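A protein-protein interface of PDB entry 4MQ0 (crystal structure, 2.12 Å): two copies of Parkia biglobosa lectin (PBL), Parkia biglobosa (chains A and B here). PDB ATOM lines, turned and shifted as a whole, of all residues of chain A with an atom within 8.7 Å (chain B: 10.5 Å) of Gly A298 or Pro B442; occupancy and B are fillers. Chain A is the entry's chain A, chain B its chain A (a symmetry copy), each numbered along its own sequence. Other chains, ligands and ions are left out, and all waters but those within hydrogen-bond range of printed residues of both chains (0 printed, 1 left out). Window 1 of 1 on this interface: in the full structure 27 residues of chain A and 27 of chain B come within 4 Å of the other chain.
Pro B442 touches Gly A298 (CB to O, 3.6 Å).
CD1 of Ile A300 touches CD1 of Ile B300 (3.3 Å).
O of His B418 touches CG2 of Ile A300, 3.7 Å away.
Ile A300 touches Lys B441.
Ile A300 touches Pro B442 (CD1 to CD, 3.7 Å).
Ile B417 touches Ser A301 (CA to O, 3.3 Å).
CB of Ser A301 touches OD1 of Asn B419, 3.4 Å away.
Lys A441 touches Ile B300 (C to CD1, 3.6 Å).
O of Gly B298 touches CB of Pro A442 (3.6 Å).
CD of Pro A442 touches CD1 of Ile B300, 3.7 Å away.
Gly A298 touches just one residue of chain B: Pro B442 (3.6 Å).
Ser A299 touches just one residue of chain B: Asn B419 (3.7 Å).
Of the printed residues of chain A, Gly B298 touches Pro A442 (3.6 Å).
Of the printed residues of chain A, Asn B420 touches Ile A300 (3.7 Å).
Printed residues of chain A within 4 Å of Lys B441: Ile A300 (3.6 Å).
Of the printed residues of chain B, Val A440 touches Ile B300.
Of the printed residues of chain B, Ser A301 touches Ile B417 (3.3 Å), His B418 (2.8 Å) and Asn B419 (3.4 Å).
Asp B295 touches none of the printed residues of chain A.
The backbone carbonyl oxygen (O) of Ser A301 lies within hydrogen-bond range of the backbone NH (N) of His B418.
Printed residues of chain A that touch a printed residue of chain B: Gly A298, Ser A299, Ile A300, Ser A301, Val A440, Lys A441 and Pro A442.
Hydrophobic or aromatic side chains of chain A that line the printed part of chain B: Ile A300, Val A440 and Pro A442.
Among the printed residues, no Asp or Glu carboxylate lies within 4 Å of a Lys or Arg side-chain nitrogen of the other chain.
Ile A300 touches its own counterpart, Ile B300.
Ile A300 touches Val B440, and with the chains exchanged Val A440 touches Ile B300.
Ile A300 touches Lys B441, and with the chains exchanged Lys A441 touches Ile B300.
Ile A300 touches Pro B442, and with the chains exchanged Pro A442 touches Ile B300.
11 positions are printed for both chains.
Of the 16 pairs that touch across the chains among the printed residues, 9 have their exchanged pair printed and touching as well.
O of Ile A300 is in hydrogen-bond range of N of Val A440.
OD2 of Asp A295 is in salt-bridge range of NZ of Lys A441.
The side-chain carboxylate (OD2) of Asp B295 lies within salt-bridge range of the side-chain amino group (NZ) of Lys B441, at 3.7 Å.
O of Ile B300 is in hydrogen-bond range of N of Val B440 (2.8 Å).
The backbone NH (N) of Asp B443 lies within hydrogen-bond range of the backbone carbonyl oxygen (O) of Asn B419.
The backbone carbonyl oxygen of Lys B441 sits at hydrogen-bond distance from the backbone NH of Met B421 (2.8 Å).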
ATOM      1  N   ARG A 294     -10.158 -11.875 -23.952  1.00  0.00           N
ATOM      2  CA  ARG A 294     -11.360 -12.292 -24.614  1.00  0.00           C
ATOM      3  C   ARG A 294     -11.791 -13.534 -23.897  1.00  0.00           C
ATOM      4  O   ARG A 294     -11.735 -14.613 -24.449  1.00  0.00           O
ATOM      5  CB  ARG A 294     -11.075 -12.657 -26.061  1.00  0.00           C
ATOM      6  CG  ARG A 294     -11.217 -11.553 -27.060  1.00  0.00           C
ATOM      7  CD  ARG A 294     -12.662 -11.131 -27.270  1.00  0.00           C
ATOM      8  NE  ARG A 294     -13.387 -12.001 -28.184  1.00  0.00           N
ATOM      9  CZ  ARG A 294     -14.434 -12.728 -27.839  1.00  0.00           C
ATOM     10  NH1 ARG A 294     -14.885 -12.692 -26.605  1.00  0.00           N
ATOM     11  NH2 ARG A 294     -15.023 -13.488 -28.724  1.00  0.00           N
ATOM     12  N   ASP A 295     -12.200 -13.385 -22.643  1.00  0.00           N
ATOM     13  CA  ASP A 295     -12.497 -14.538 -21.803  1.00  0.00           C
ATOM     14  C   ASP A 295     -13.416 -15.521 -22.513  1.00  0.00           C
ATOM     15  O   ASP A 295     -12.948 -16.380 -23.222  1.00  0.00           O
ATOM     16  CB  ASP A 295     -13.113 -14.127 -20.465  1.00  0.00           C
ATOM     17  CG  ASP A 295     -14.601 -14.043 -20.540  1.00  0.00           C
ATOM     18  OD1 ASP A 295     -15.097 -13.874 -21.651  1.00  0.00           O
ATOM     19  OD2 ASP A 295     -15.282 -14.153 -19.515  1.00  0.00           O
ATOM     20  N   GLY A 298     -18.906 -16.320 -21.322  1.00  0.00           N
ATOM     21  CA  GLY A 298     -20.193 -15.756 -21.760  1.00  0.00           C
ATOM     22  C   GLY A 298     -21.125 -15.605 -20.563  1.00  0.00           C
ATOM     23  O   GLY A 298     -20.981 -16.320 -19.553  1.00  0.00           O
ATOM     24  N   SER A 299     -22.055 -14.653 -20.646  1.00  0.00           N
ATOM     25  CA  SER A 299     -23.062 -14.491 -19.596  1.00  0.00           C
ATOM     26  C   SER A 299     -24.375 -14.950 -20.186  1.00  0.00           C
ATOM     27  O   SER A 299     -24.560 -14.896 -21.423  1.00  0.00           O
ATOM     28  CB  SER A 299     -23.248 -13.034 -19.175  1.00  0.00           C
ATOM     29  OG  SER A 299     -22.163 -12.215 -19.556  1.00  0.00           O
ATOM     30  N   ILE A 300     -25.285 -15.360 -19.301  1.00  0.00           N
ATOM     31  CA  ILE A 300     -26.690 -15.507 -19.675  1.00  0.00           C
ATOM     32  C   ILE A 300     -27.367 -14.181 -19.481  1.00  0.00           C
ATOM     33  O   ILE A 300     -27.016 -13.430 -18.567  1.00  0.00           O
ATOM     34  CB  ILE A 300     -27.438 -16.498 -18.786  1.00  0.00           C
ATOM     35  CG1 ILE A 300     -26.949 -17.906 -19.076  1.00  0.00           C
ATOM     36  CG2 ILE A 300     -28.970 -16.368 -18.980  1.00  0.00           C
ATOM     37  CD1 ILE A 300     -26.930 -18.795 -17.881  1.00  0.00           C
ATOM     38  N   SER A 301     -28.356 -13.913 -20.330  1.00  0.00           N
ATOM     39  CA  SER A 301     -29.024 -12.642 -20.318  1.00  0.00           C
ATOM     40  C   SER A 301     -30.466 -12.805 -19.899  1.00  0.00           C
ATOM     41  O   SER A 301     -31.183 -13.627 -20.466  1.00  0.00           O
ATOM     42  CB  SER A 301     -28.960 -12.012 -21.700  1.00  0.00           C
ATOM     43  OG  SER A 301     -30.010 -11.087 -21.786  1.00  0.00           O
ATOM     44  N   THR A 316     -21.002  -4.798 -18.227  1.00  0.00           N
ATOM     45  CA  THR A 316     -20.454  -5.963 -17.600  1.00  0.00           C
ATOM     46  C   THR A 316     -19.285  -5.538 -16.710  1.00  0.00           C
ATOM     47  O   THR A 316     -18.364  -4.851 -17.158  1.00  0.00           O
ATOM     48  CB  THR A 316     -19.970  -6.969 -18.622  1.00  0.00           C
ATOM     49  OG1 THR A 316     -21.074  -7.348 -19.456  1.00  0.00           O
ATOM     50  CG2 THR A 316     -19.420  -8.200 -17.891  1.00  0.00           C
ATOM     51  N   VAL A 423     -23.552 -10.336 -13.072  1.00  0.00           N
ATOM     52  CA  VAL A 423     -22.196  -9.873 -13.509  1.00  0.00           C
ATOM     53  C   VAL A 423     -22.260  -8.598 -14.343  1.00  0.00           C
ATOM     54  O   VAL A 423     -21.218  -8.089 -14.849  1.00  0.00           O
ATOM     55  CB  VAL A 423     -21.390 -10.928 -14.346  1.00  0.00           C
ATOM     56  CG1 VAL A 423     -20.958 -12.138 -13.514  1.00  0.00           C
ATOM     57  CG2 VAL A 423     -22.110 -11.318 -15.677  1.00  0.00           C
ATOM     58  N   PHE A 439     -27.327  -9.713 -16.447  1.00  0.00           N
ATOM     59  CA  PHE A 439     -26.489 -10.715 -17.027  1.00  0.00           C
ATOM     60  C   PHE A 439     -26.096 -11.549 -15.830  1.00  0.00           C
ATOM     61  O   PHE A 439     -25.746 -10.962 -14.789  1.00  0.00           O
ATOM     62  CB  PHE A 439     -25.186 -10.109 -17.592  1.00  0.00           C
ATOM     63  CG  PHE A 439     -25.350  -9.400 -18.940  1.00  0.00           C
ATOM     64  CD1 PHE A 439     -25.005  -8.062 -19.075  1.00  0.00           C
ATOM     65  CD2 PHE A 439     -25.869 -10.079 -20.045  1.00  0.00           C
ATOM     66  CE1 PHE A 439     -25.155  -7.409 -20.273  1.00  0.00           C
ATOM     67  CE2 PHE A 439     -26.039  -9.434 -21.243  1.00  0.00           C
ATOM     68  CZ  PHE A 439     -25.673  -8.097 -21.369  1.00  0.00           C
ATOM     69  N   VAL A 440     -26.106 -12.879 -15.966  1.00  0.00           N
ATOM     70  CA  VAL A 440     -25.774 -13.766 -14.836  1.00  0.00           C
ATOM     71  C   VAL A 440     -24.799 -14.884 -15.230  1.00  0.00           C
ATOM     72  O   VAL A 440     -24.693 -15.236 -16.402  1.00  0.00           O
ATOM     73  CB  VAL A 440     -27.034 -14.442 -14.167  1.00  0.00           C
ATOM     74  CG1 VAL A 440     -28.023 -13.391 -13.593  1.00  0.00           C
ATOM     75  CG2 VAL A 440     -27.742 -15.361 -15.113  1.00  0.00           C
ATOM     76  N   LYS A 441     -24.128 -15.415 -14.243  1.00  0.00           N
ATOM     77  CA  LYS A 441     -23.242 -16.525 -14.412  1.00  0.00           C
ATOM     78  C   LYS A 441     -23.466 -17.412 -13.233  1.00  0.00           C
ATOM     79  O   LYS A 441     -24.044 -17.001 -12.273  1.00  0.00           O
ATOM     80  CB  LYS A 441     -21.820 -16.042 -14.414  1.00  0.00           C
ATOM     81  CG  LYS A 441     -21.304 -15.701 -15.762  1.00  0.00           C
ATOM     82  CD  LYS A 441     -19.894 -15.261 -15.680  1.00  0.00           C
ATOM     83  CE  LYS A 441     -19.287 -15.155 -17.028  1.00  0.00           C
ATOM     84  NZ  LYS A 441     -17.855 -14.839 -16.958  1.00  0.00           N
ATOM     85  N   PRO A 442     -22.987 -18.632 -13.305  1.00  0.00           N
ATOM     86  CA  PRO A 442     -23.241 -19.626 -12.284  1.00  0.00           C
ATOM     87  C   PRO A 442     -22.403 -19.463 -11.071  1.00  0.00           C
ATOM     88  O   PRO A 442     -21.613 -18.573 -10.970  1.00  0.00           O
ATOM     89  CB  PRO A 442     -22.832 -20.900 -12.975  1.00  0.00           C
ATOM     90  CG  PRO A 442     -23.098 -20.661 -14.338  1.00  0.00           C
ATOM     91  CD  PRO A 442     -22.891 -19.249 -14.624  1.00  0.00           C
ATOM     92  N   ASP A 443     -22.594 -20.383 -10.154  1.00  0.00           N
ATOM     93  CA  ASP A 443     -21.801 -20.543  -8.942  1.00  0.00           C
ATOM     94  C   ASP A 443     -22.441 -19.754  -7.844  1.00  0.00           C
ATOM     95  O   ASP A 443     -22.444 -18.557  -7.933  1.00  0.00           O
ATOM     96  CB  ASP A 443     -20.356 -20.104  -9.149  1.00  0.00           C
ATOM     97  CG  ASP A 443     -19.418 -21.268  -9.316  1.00  0.00           C
ATOM     98  OD1 ASP A 443     -19.883 -22.422  -9.308  1.00  0.00           O
ATOM     99  OD2 ASP A 443     -18.205 -21.034  -9.461  1.00  0.00           O
ATOM    100  N   ASP B 295     -17.092 -32.038 -12.720  1.00  0.00           N
ATOM    101  CA  ASP B 295     -16.834 -30.871 -13.554  1.00  0.00           C
ATOM    102  C   ASP B 295     -16.831 -29.591 -12.735  1.00  0.00           C
ATOM    103  O   ASP B 295     -15.811 -29.217 -12.205  1.00  0.00           O
ATOM    104  CB  ASP B 295     -17.843 -30.753 -14.698  1.00  0.00           C
ATOM    105  CG  ASP B 295     -19.043 -29.960 -14.300  1.00  0.00           C
ATOM    106  OD1 ASP B 295     -19.292 -29.886 -13.099  1.00  0.00           O
ATOM    107  OD2 ASP B 295     -19.734 -29.403 -15.160  1.00  0.00           O
ATOM    108  N   GLY B 298     -20.927 -25.664 -12.774  1.00  0.00           N
ATOM    109  CA  GLY B 298     -22.171 -25.402 -12.032  1.00  0.00           C
ATOM    110  C   GLY B 298     -23.246 -24.899 -12.988  1.00  0.00           C
ATOM    111  O   GLY B 298     -22.934 -24.332 -14.053  1.00  0.00           O
ATOM    112  N   SER B 299     -24.512 -25.134 -12.641  1.00  0.00           N
ATOM    113  CA  SER B 299     -25.622 -24.606 -13.437  1.00  0.00           C
ATOM    114  C   SER B 299     -26.258 -23.512 -12.613  1.00  0.00           C
ATOM    115  O   SER B 299     -26.170 -23.534 -11.364  1.00  0.00           O
ATOM    116  CB  SER B 299     -26.706 -25.649 -13.706  1.00  0.00           C
ATOM    117  OG  SER B 299     -26.250 -26.970 -13.510  1.00  0.00           O
ATOM    118  N   ILE B 300     -26.923 -22.587 -13.308  1.00  0.00           N
ATOM    119  CA  ILE B 300     -27.859 -21.676 -12.653  1.00  0.00           C
ATOM    120  C   ILE B 300     -29.204 -22.344 -12.605  1.00  0.00           C
ATOM    121  O   ILE B 300     -29.561 -23.093 -13.518  1.00  0.00           O
ATOM    122  CB  ILE B 300     -28.059 -20.376 -13.429  1.00  0.00           C
ATOM    123  CG1 ILE B 300     -26.795 -19.540 -13.349  1.00  0.00           C
ATOM    124  CG2 ILE B 300     -29.295 -19.603 -12.902  1.00  0.00           C
ATOM    125  CD1 ILE B 300     -26.518 -18.748 -14.580  1.00  0.00           C
ATOM    126  N   SER B 301     -29.953 -22.044 -11.547  1.00  0.00           N
ATOM    127  CA  SER B 301     -31.219 -22.684 -11.327  1.00  0.00           C
ATOM    128  C   SER B 301     -32.346 -21.684 -11.437  1.00  0.00           C
ATOM    129  O   SER B 301     -32.308 -20.641 -10.789  1.00  0.00           O
ATOM    130  CB  SER B 301     -31.240 -23.328  -9.950  1.00  0.00           C
ATOM    131  OG  SER B 301     -32.583 -23.472  -9.576  1.00  0.00           O
ATOM    132  N   ILE B 302     -33.358 -22.010 -12.231  1.00  0.00           N
ATOM    133  CA  ILE B 302     -34.502 -21.126 -12.357  1.00  0.00           C
ATOM    134  C   ILE B 302     -35.819 -21.811 -12.007  1.00  0.00           C
ATOM    135  O   ILE B 302     -36.099 -22.897 -12.478  1.00  0.00           O
ATOM    136  CB  ILE B 302     -34.565 -20.450 -13.783  1.00  0.00           C
ATOM    137  CG1 ILE B 302     -33.134 -20.098 -14.264  1.00  0.00           C
ATOM    138  CG2 ILE B 302     -35.546 -19.284 -13.761  1.00  0.00           C
ATOM    139  CD1 ILE B 302     -32.999 -18.949 -15.217  1.00  0.00           C
ATOM    140  N   TYR B 370     -31.050 -26.857 -29.448  1.00  0.00           N
ATOM    141  CA  TYR B 370     -30.887 -27.164 -28.042  1.00  0.00           C
ATOM    142  C   TYR B 370     -31.932 -26.356 -27.252  1.00  0.00           C
ATOM    143  O   TYR B 370     -32.318 -25.242 -27.674  1.00  0.00           O
ATOM    144  CB  TYR B 370     -29.436 -26.879 -27.574  1.00  0.00           C
ATOM    145  CG  TYR B 370     -28.961 -25.511 -27.981  1.00  0.00           C
ATOM    146  CD1 TYR B 370     -29.259 -24.408 -27.195  1.00  0.00           C
ATOM    147  CD2 TYR B 370     -28.249 -25.315 -29.158  1.00  0.00           C
ATOM    148  CE1 TYR B 370     -28.871 -23.127 -27.541  1.00  0.00           C
ATOM    149  CE2 TYR B 370     -27.836 -24.028 -29.524  1.00  0.00           C
ATOM    150  CZ  TYR B 370     -28.174 -22.932 -28.702  1.00  0.00           C
ATOM    151  OH  TYR B 370     -27.792 -21.660 -28.999  1.00  0.00           O
ATOM    152  N   LEU B 371     -32.404 -26.875 -26.122  1.00  0.00           N
ATOM    153  CA  LEU B 371     -33.483 -26.204 -25.389  1.00  0.00           C
ATOM    154  C   LEU B 371     -33.058 -24.839 -24.834  1.00  0.00           C
ATOM    155  O   LEU B 371     -31.964 -24.701 -24.285  1.00  0.00           O
ATOM    156  CB  LEU B 371     -33.993 -27.094 -24.253  1.00  0.00           C
ATOM    157  CG  LEU B 371     -34.571 -28.450 -24.663  1.00  0.00           C
ATOM    158  CD1 LEU B 371     -34.960 -29.262 -23.437  1.00  0.00           C
ATOM    159  CD2 LEU B 371     -35.763 -28.268 -25.590  1.00  0.00           C
ATOM    160  N   THR B 372     -33.923 -23.833 -24.981  1.00  0.00           N
ATOM    161  CA  THR B 372     -33.655 -22.498 -24.430  1.00  0.00           C
ATOM    162  C   THR B 372     -34.384 -22.168 -23.119  1.00  0.00           C
ATOM    163  O   THR B 372     -33.778 -21.662 -22.175  1.00  0.00           O
ATOM    164  CB  THR B 372     -33.971 -21.396 -25.461  1.00  0.00           C
ATOM    165  OG1 THR B 372     -33.165 -21.586 -26.631  1.00  0.00           O
ATOM    166  CG2 THR B 372     -33.689 -20.022 -24.875  1.00  0.00           C
ATOM    167  N   ILE B 417     -35.274 -15.187 -21.227  1.00  0.00           N
ATOM    168  CA  ILE B 417     -33.846 -15.530 -21.063  1.00  0.00           C
ATOM    169  C   ILE B 417     -33.195 -15.697 -22.439  1.00  0.00           C
ATOM    170  O   ILE B 417     -33.864 -16.131 -23.344  1.00  0.00           O
ATOM    171  CB  ILE B 417     -33.727 -16.850 -20.254  1.00  0.00           C
ATOM    172  CG1 ILE B 417     -32.274 -17.249 -20.012  1.00  0.00           C
ATOM    173  CG2 ILE B 417     -34.410 -17.980 -20.993  1.00  0.00           C
ATOM    174  CD1 ILE B 417     -32.048 -18.144 -18.805  1.00  0.00           C
ATOM    175  N   HIS B 418     -31.903 -15.350 -22.600  1.00  0.00           N
ATOM    176  CA  HIS B 418     -31.203 -15.415 -23.890  1.00  0.00           C
ATOM    177  C   HIS B 418     -29.726 -15.792 -23.698  1.00  0.00           C
ATOM    178  O   HIS B 418     -29.190 -15.731 -22.586  1.00  0.00           O
ATOM    179  CB  HIS B 418     -31.313 -14.093 -24.666  1.00  0.00           C
ATOM    180  CG  HIS B 418     -32.709 -13.532 -24.743  1.00  0.00           C
ATOM    181  ND1 HIS B 418     -33.659 -14.027 -25.609  1.00  0.00           N
ATOM    182  CD2 HIS B 418     -33.315 -12.537 -24.050  1.00  0.00           C
ATOM    183  CE1 HIS B 418     -34.794 -13.371 -25.435  1.00  0.00           C
ATOM    184  NE2 HIS B 418     -34.608 -12.458 -24.494  1.00  0.00           N
ATOM    185  N   ASN B 419     -29.067 -16.181 -24.781  1.00  0.00           N
ATOM    186  CA  ASN B 419     -27.627 -16.596 -24.767  1.00  0.00           C
ATOM    187  C   ASN B 419     -27.360 -17.731 -23.771  1.00  0.00           C
ATOM    188  O   ASN B 419     -26.334 -17.756 -23.094  1.00  0.00           O
ATOM    189  CB  ASN B 419     -26.649 -15.427 -24.461  1.00  0.00           C
ATOM    190  CG  ASN B 419     -27.135 -14.035 -24.998  1.00  0.00           C
ATOM    191  OD1 ASN B 419     -27.008 -13.023 -24.310  1.00  0.00           O
ATOM    192  ND2 ASN B 419     -27.641 -14.000 -26.216  1.00  0.00           N
ATOM    193  N   ASN B 420     -28.301 -18.656 -23.655  1.00  0.00           N
ATOM    194  CA  ASN B 420     -28.154 -19.774 -22.697  1.00  0.00           C
ATOM    195  C   ASN B 420     -28.446 -21.117 -23.343  1.00  0.00           C
ATOM    196  O   ASN B 420     -28.818 -21.175 -24.518  1.00  0.00           O
ATOM    197  CB  ASN B 420     -29.159 -19.600 -21.560  1.00  0.00           C
ATOM    198  CG  ASN B 420     -30.585 -19.690 -22.045  1.00  0.00           C
ATOM    199  OD1 ASN B 420     -30.962 -18.966 -22.941  1.00  0.00           O
ATOM    200  ND2 ASN B 420     -31.364 -20.632 -21.506  1.00  0.00           N
ATOM    201  N   MET B 421     -28.296 -22.197 -22.565  1.00  0.00           N
ATOM    202  CA  MET B 421     -28.965 -23.454 -22.876  1.00  0.00           C
ATOM    203  C   MET B 421     -29.462 -24.144 -21.634  1.00  0.00           C
ATOM    204  O   MET B 421     -28.868 -24.014 -20.557  1.00  0.00           O
ATOM    205  CB  MET B 421     -28.121 -24.383 -23.751  1.00  0.00           C
ATOM    206  CG  MET B 421     -26.800 -24.803 -23.155  1.00  0.00           C
ATOM    207  SD  MET B 421     -25.674 -25.288 -24.499  1.00  0.00           S
ATOM    208  CE  MET B 421     -26.582 -26.654 -25.256  1.00  0.00           C
ATOM    209  N   VAL B 422     -30.591 -24.821 -21.775  1.00  0.00           N
ATOM    210  CA  VAL B 422     -31.160 -25.604 -20.670  1.00  0.00           C
ATOM    211  C   VAL B 422     -30.352 -26.898 -20.577  1.00  0.00           C
ATOM    212  O   VAL B 422     -30.165 -27.567 -21.594  1.00  0.00           O
ATOM    213  CB  VAL B 422     -32.660 -25.852 -20.939  1.00  0.00           C
ATOM    214  CG1 VAL B 422     -33.258 -26.862 -19.951  1.00  0.00           C
ATOM    215  CG2 VAL B 422     -33.438 -24.517 -20.888  1.00  0.00           C
ATOM    216  N   VAL B 423     -29.823 -27.231 -19.397  1.00  0.00           N
ATOM    217  CA  VAL B 423     -28.936 -28.426 -19.230  1.00  0.00           C
ATOM    218  C   VAL B 423     -29.549 -29.480 -18.315  1.00  0.00           C
ATOM    219  O   VAL B 423     -28.918 -30.533 -18.009  1.00  0.00           O
ATOM    220  CB  VAL B 423     -27.509 -28.099 -18.661  1.00  0.00           C
ATOM    221  CG1 VAL B 423     -26.645 -27.312 -19.649  1.00  0.00           C
ATOM    222  CG2 VAL B 423     -27.562 -27.457 -17.238  1.00  0.00           C
ATOM    223  N   PHE B 439     -32.423 -25.774 -15.257  1.00  0.00           N
ATOM    224  CA  PHE B 439     -31.058 -25.490 -14.941  1.00  0.00           C
ATOM    225  C   PHE B 439     -30.522 -24.961 -16.250  1.00  0.00           C
ATOM    226  O   PHE B 439     -30.811 -25.567 -17.298  1.00  0.00           O
ATOM    227  CB  PHE B 439     -30.268 -26.779 -14.628  1.00  0.00           C
ATOM    228  CG  PHE B 439     -30.520 -27.352 -13.229  1.00  0.00           C
ATOM    229  CD1 PHE B 439     -30.999 -28.647 -13.078  1.00  0.00           C
ATOM    230  CD2 PHE B 439     -30.296 -26.579 -12.090  1.00  0.00           C
ATOM    231  CE1 PHE B 439     -31.240 -29.172 -11.833  1.00  0.00           C
ATOM    232  CE2 PHE B 439     -30.547 -27.085 -10.840  1.00  0.00           C
ATOM    233  CZ  PHE B 439     -31.011 -28.391 -10.704  1.00  0.00           C
ATOM    234  N   VAL B 440     -29.726 -23.887 -16.208  1.00  0.00           N
ATOM    235  CA  VAL B 440     -29.191 -23.281 -17.443  1.00  0.00           C
ATOM    236  C   VAL B 440     -27.691 -22.971 -17.346  1.00  0.00           C
ATOM    237  O   VAL B 440     -27.151 -22.829 -16.251  1.00  0.00           O
ATOM    238  CB  VAL B 440     -29.930 -21.955 -17.872  1.00  0.00           C
ATOM    239  CG1 VAL B 440     -31.440 -22.189 -18.145  1.00  0.00           C
ATOM    240  CG2 VAL B 440     -29.747 -20.863 -16.863  1.00  0.00           C
ATOM    241  N   LYS B 441     -27.068 -22.863 -18.489  1.00  0.00           N
ATOM    242  CA  LYS B 441     -25.690 -22.491 -18.592  1.00  0.00           C
ATOM    243  C   LYS B 441     -25.603 -21.560 -19.754  1.00  0.00           C
ATOM    244  O   LYS B 441     -26.500 -21.488 -20.537  1.00  0.00           O
ATOM    245  CB  LYS B 441     -24.855 -23.709 -18.860  1.00  0.00           C
ATOM    246  CG  LYS B 441     -24.361 -24.381 -17.634  1.00  0.00           C
ATOM    247  CD  LYS B 441     -23.528 -25.552 -17.985  1.00  0.00           C
ATOM    248  CE  LYS B 441     -22.824 -26.085 -16.794  1.00  0.00           C
ATOM    249  NZ  LYS B 441     -21.901 -27.171 -17.148  1.00  0.00           N
ATOM    250  N   PRO B 442     -24.501 -20.856 -19.872  1.00  0.00           N
ATOM    251  CA  PRO B 442     -24.341 -19.830 -20.882  1.00  0.00           C
ATOM    252  C   PRO B 442     -24.038 -20.366 -22.232  1.00  0.00           C
ATOM    253  O   PRO B 442     -23.958 -21.539 -22.437  1.00  0.00           O
ATOM    254  CB  PRO B 442     -23.129 -19.084 -20.385  1.00  0.00           C
ATOM    255  CG  PRO B 442     -23.186 -19.218 -18.984  1.00  0.00           C
ATOM    256  CD  PRO B 442     -23.784 -20.503 -18.651  1.00  0.00           C
ATOM    257  N   ASP B 443     -23.849 -19.446 -23.148  1.00  0.00           N
ATOM    258  CA  ASP B 443     -23.393 -19.692 -24.510  1.00  0.00           C
ATOM    259  C   ASP B 443     -24.590 -19.882 -25.387  1.00  0.00           C
ATOM    260  O   ASP B 443     -25.270 -20.856 -25.217  1.00  0.00           O
ATOM    261  CB  ASP B 443     -22.471 -20.904 -24.587  1.00  0.00           C
ATOM    262  CG  ASP B 443     -21.022 -20.519 -24.708  1.00  0.00           C
ATOM    263  OD1 ASP B 443     -20.717 -19.312 -24.696  1.00  0.00           O
ATOM    264  OD2 ASP B 443     -20.176 -21.425 -24.810  1.00  0.00           O
